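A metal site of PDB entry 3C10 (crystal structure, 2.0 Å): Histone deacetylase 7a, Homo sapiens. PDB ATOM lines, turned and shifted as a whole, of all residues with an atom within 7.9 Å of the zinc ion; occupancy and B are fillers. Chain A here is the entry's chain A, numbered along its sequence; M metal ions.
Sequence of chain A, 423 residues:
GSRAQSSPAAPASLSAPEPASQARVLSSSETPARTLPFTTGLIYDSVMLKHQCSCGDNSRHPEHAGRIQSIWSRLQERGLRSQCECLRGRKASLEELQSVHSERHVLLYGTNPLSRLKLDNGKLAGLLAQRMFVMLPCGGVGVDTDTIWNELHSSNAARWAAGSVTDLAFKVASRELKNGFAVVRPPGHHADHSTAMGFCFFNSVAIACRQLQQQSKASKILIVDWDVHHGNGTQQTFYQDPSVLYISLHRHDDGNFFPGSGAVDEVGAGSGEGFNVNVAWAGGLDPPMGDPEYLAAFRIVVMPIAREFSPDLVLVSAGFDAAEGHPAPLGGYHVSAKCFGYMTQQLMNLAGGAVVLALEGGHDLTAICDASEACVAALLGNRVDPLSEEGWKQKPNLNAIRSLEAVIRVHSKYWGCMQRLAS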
ATOM      1  N   GLN A  52     -13.956  28.894  23.919  1.00  0.00           N
ATOM      2  CA  GLN A  52     -15.065  29.561  24.590  1.00  0.00           C
ATOM      3  C   GLN A  52     -16.119  28.515  24.821  1.00  0.00           C
ATOM      4  O   GLN A  52     -16.337  27.653  23.956  1.00  0.00           O
ATOM      5  CB  GLN A  52     -15.680  30.690  23.718  1.00  0.00           C
ATOM      6  CG  GLN A  52     -14.686  31.719  23.136  1.00  0.00           C
ATOM      7  CD  GLN A  52     -15.309  32.666  22.089  1.00  0.00           C
ATOM      8  OE1 GLN A  52     -14.600  33.408  21.406  1.00  0.00           O
ATOM      9  NE2 GLN A  52     -16.633  32.630  21.952  1.00  0.00           N
ATOM     10  N   CYS A  53     -16.751  28.575  25.980  1.00  0.00           N
ATOM     11  CA  CYS A  53     -17.916  27.722  26.233  1.00  0.00           C
ATOM     12  C   CYS A  53     -18.987  27.979  25.164  1.00  0.00           C
ATOM     13  O   CYS A  53     -19.110  29.117  24.608  1.00  0.00           O
ATOM     14  CB  CYS A  53     -18.468  27.941  27.633  1.00  0.00           C
ATOM     15  SG  CYS A  53     -19.653  26.678  28.117  1.00  0.00           S
ATOM     16  N   SER A  54     -19.728  26.927  24.853  1.00  0.00           N
ATOM     17  CA  SER A  54     -20.850  27.035  23.915  1.00  0.00           C
ATOM     18  C   SER A  54     -22.063  27.833  24.474  1.00  0.00           C
ATOM     19  O   SER A  54     -22.998  28.137  23.720  1.00  0.00           O
ATOM     20  CB  SER A  54     -21.293  25.652  23.452  1.00  0.00           C
ATOM     21  OG  SER A  54     -21.345  24.777  24.569  1.00  0.00           O
ATOM     22  N   CYS A  55     -22.051  28.147  25.774  1.00  0.00           N
ATOM     23  CA  CYS A  55     -23.141  28.917  26.420  1.00  0.00           C
ATOM     24  C   CYS A  55     -23.090  30.404  26.096  1.00  0.00           C
ATOM     25  O   CYS A  55     -24.040  31.134  26.388  1.00  0.00           O
ATOM     26  CB  CYS A  55     -23.137  28.726  27.932  1.00  0.00           C
ATOM     27  SG  CYS A  55     -21.935  29.781  28.752  1.00  0.00           S
ATOM     28  N   GLY A  56     -21.995  30.857  25.487  1.00  0.00           N
ATOM     29  CA  GLY A  56     -21.862  32.240  25.029  1.00  0.00           C
ATOM     30  C   GLY A  56     -21.936  33.292  26.123  1.00  0.00           C
ATOM     31  O   GLY A  56     -22.352  34.410  25.872  1.00  0.00           O
ATOM     32  N   ASP A  57     -21.553  32.935  27.353  1.00  0.00           N
ATOM     33  CA  ASP A  57     -21.644  33.851  28.497  1.00  0.00           C
ATOM     34  C   ASP A  57     -20.313  34.006  29.251  1.00  0.00           C
ATOM     35  O   ASP A  57     -19.979  33.188  30.107  1.00  0.00           O
ATOM     36  CB  ASP A  57     -22.730  33.362  29.458  1.00  0.00           C
ATOM     37  CG  ASP A  57     -23.227  34.449  30.399  1.00  0.00           C
ATOM     38  OD1 ASP A  57     -22.830  35.636  30.238  1.00  0.00           O
ATOM     39  OD2 ASP A  57     -24.035  34.111  31.295  1.00  0.00           O
ATOM     40  N   ASN A  58     -19.558  35.048  28.909  1.00  0.00           N
ATOM     41  CA  ASN A  58     -18.343  35.406  29.639  1.00  0.00           C
ATOM     42  C   ASN A  58     -18.588  35.655  31.135  1.00  0.00           C
ATOM     43  O   ASN A  58     -17.647  35.657  31.920  1.00  0.00           O
ATOM     44  CB  ASN A  58     -17.716  36.666  29.042  1.00  0.00           C
ATOM     45  CG  ASN A  58     -17.111  36.434  27.692  1.00  0.00           C
ATOM     46  OD1 ASN A  58     -16.987  35.292  27.227  1.00  0.00           O
ATOM     47  ND2 ASN A  58     -16.700  37.531  27.041  1.00  0.00           N
ATOM     48  N   ARG A  60     -20.143  33.813  33.491  1.00  0.00           N
ATOM     49  CA  ARG A  60     -19.835  32.678  34.370  1.00  0.00           C
ATOM     50  C   ARG A  60     -18.511  31.965  34.047  1.00  0.00           C
ATOM     51  O   ARG A  60     -18.230  30.908  34.623  1.00  0.00           O
ATOM     52  CB  ARG A  60     -21.006  31.681  34.411  1.00  0.00           C
ATOM     53  CG  ARG A  60     -21.652  31.358  33.087  1.00  0.00           C
ATOM     54  CD  ARG A  60     -22.867  30.461  33.311  1.00  0.00           C
ATOM     55  NE  ARG A  60     -23.644  30.260  32.083  1.00  0.00           N
ATOM     56  CZ  ARG A  60     -24.853  30.744  31.845  1.00  0.00           C
ATOM     57  NH1 ARG A  60     -25.491  31.487  32.747  1.00  0.00           N
ATOM     58  NH2 ARG A  60     -25.452  30.485  30.688  1.00  0.00           N
ATOM     59  N   HIS A  61     -17.729  32.552  33.145  1.00  0.00           N
ATOM     60  CA  HIS A  61     -16.466  31.986  32.658  1.00  0.00           C
ATOM     61  C   HIS A  61     -15.363  33.052  32.599  1.00  0.00           C
ATOM     62  O   HIS A  61     -15.114  33.606  31.535  1.00  0.00           O
ATOM     63  CB  HIS A  61     -16.648  31.344  31.269  1.00  0.00           C
ATOM     64  CG  HIS A  61     -17.729  30.305  31.209  1.00  0.00           C
ATOM     65  ND1 HIS A  61     -17.710  29.162  31.985  1.00  0.00           N
ATOM     66  CD2 HIS A  61     -18.840  30.213  30.436  1.00  0.00           C
ATOM     67  CE1 HIS A  61     -18.780  28.432  31.723  1.00  0.00           C
ATOM     68  NE2 HIS A  61     -19.478  29.048  30.784  1.00  0.00           N
ATOM     69  N   LEU A 136     -21.788  20.877  32.256  1.00  0.00           N
ATOM     70  CA  LEU A 136     -21.741  22.047  33.102  1.00  0.00           C
ATOM     71  C   LEU A 136     -23.178  22.547  33.344  1.00  0.00           C
ATOM     72  O   LEU A 136     -24.099  22.203  32.582  1.00  0.00           O
ATOM     73  CB  LEU A 136     -20.830  23.138  32.495  1.00  0.00           C
ATOM     74  CG  LEU A 136     -19.352  22.737  32.379  1.00  0.00           C
ATOM     75  CD1 LEU A 136     -18.529  23.861  31.731  1.00  0.00           C
ATOM     76  CD2 LEU A 136     -18.736  22.347  33.716  1.00  0.00           C
ATOM     77  N   PRO A 137     -23.376  23.320  34.435  1.00  0.00           N
ATOM     78  CA  PRO A 137     -24.659  23.953  34.714  1.00  0.00           C
ATOM     79  C   PRO A 137     -25.156  24.756  33.526  1.00  0.00           C
ATOM     80  O   PRO A 137     -26.372  24.781  33.286  1.00  0.00           O
ATOM     81  CB  PRO A 137     -24.337  24.921  35.864  1.00  0.00           C
ATOM     82  CG  PRO A 137     -23.188  24.220  36.623  1.00  0.00           C
ATOM     83  CD  PRO A 137     -22.369  23.585  35.501  1.00  0.00           C
ATOM     84  N   CYS A 138     -24.236  25.403  32.800  1.00  0.00           N
ATOM     85  CA  CYS A 138     -24.625  26.283  31.665  1.00  0.00           C
ATOM     86  C   CYS A 138     -25.037  25.504  30.402  1.00  0.00           C
ATOM     87  O   CYS A 138     -25.443  26.110  29.404  1.00  0.00           O
ATOM     88  CB  CYS A 138     -23.471  27.223  31.338  1.00  0.00           C
ATOM     89  SG  CYS A 138     -21.880  26.415  30.809  1.00  0.00           S
ATOM     90  N   GLY A 139     -24.934  24.181  30.469  1.00  0.00           N
ATOM     91  CA  GLY A 139     -25.099  23.280  29.331  1.00  0.00           C
ATOM     92  C   GLY A 139     -23.867  23.030  28.454  1.00  0.00           C
ATOM     93  O   GLY A 139     -23.914  22.225  27.528  1.00  0.00           O
ATOM     94  N   GLY A 140     -22.752  23.710  28.737  1.00  0.00           N
ATOM     95  CA  GLY A 140     -21.543  23.514  27.961  1.00  0.00           C
ATOM     96  C   GLY A 140     -20.880  22.275  28.483  1.00  0.00           C
ATOM     97  O   GLY A 140     -21.228  21.769  29.591  1.00  0.00           O
ATOM     98  N   VAL A 141     -19.938  21.759  27.716  1.00  0.00           N
ATOM     99  CA  VAL A 141     -19.159  20.608  28.145  1.00  0.00           C
ATOM    100  C   VAL A 141     -17.975  21.170  28.895  1.00  0.00           C
ATOM    101  O   VAL A 141     -17.529  22.265  28.588  1.00  0.00           O
ATOM    102  CB  VAL A 141     -18.697  19.735  26.933  1.00  0.00           C
ATOM    103  CG1 VAL A 141     -17.524  18.753  27.314  1.00  0.00           C
ATOM    104  CG2 VAL A 141     -19.863  18.961  26.442  1.00  0.00           C
ATOM    105  N   THR A 145     -16.126  21.986  36.758  1.00  0.00           N
ATOM    106  CA  THR A 145     -16.938  23.230  36.856  1.00  0.00           C
ATOM    107  C   THR A 145     -16.341  24.481  36.205  1.00  0.00           C
ATOM    108  O   THR A 145     -17.021  25.202  35.462  1.00  0.00           O
ATOM    109  CB  THR A 145     -17.293  23.565  38.362  1.00  0.00           C
ATOM    110  OG1 THR A 145     -16.128  24.024  39.063  1.00  0.00           O
ATOM    111  CG2 THR A 145     -17.865  22.348  39.077  1.00  0.00           C
ATOM    112  N   ILE A 148     -13.738  24.653  31.009  1.00  0.00           N
ATOM    113  CA  ILE A 148     -14.658  24.460  29.899  1.00  0.00           C
ATOM    114  C   ILE A 148     -13.963  23.813  28.703  1.00  0.00           C
ATOM    115  O   ILE A 148     -12.760  23.947  28.520  1.00  0.00           O
ATOM    116  CB  ILE A 148     -15.342  25.792  29.441  1.00  0.00           C
ATOM    117  CG1 ILE A 148     -14.395  26.708  28.611  1.00  0.00           C
ATOM    118  CG2 ILE A 148     -15.920  26.528  30.665  1.00  0.00           C
ATOM    119  CD1 ILE A 148     -14.401  26.447  27.061  1.00  0.00           C
HETATM  120 ZN    ZN M   1     -20.848  27.973  29.791  1.00  0.00          ZN
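The nearest printed residue that does not touch the zinc ion is Arg 60 (4.3 Å).
The zinc ion is bound by NE2 of His 61 (2.0 Å), SG of Cys 138 (2.1 Å), SG of Cys 55 (2.4 Å) and SG of Cys 53 (2.4 Å).
The guanidinium group of Arg 60 lies close to the side-chain sulfur of Cys 55 (3.8 Å).
SG of Cys 55 lies close to N of Asp 57 (3.5 Å).
The side-chain sulfur (SG) of Cys 138 sits close to the backbone NH (N) of Gly 140 (3.5 Å).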
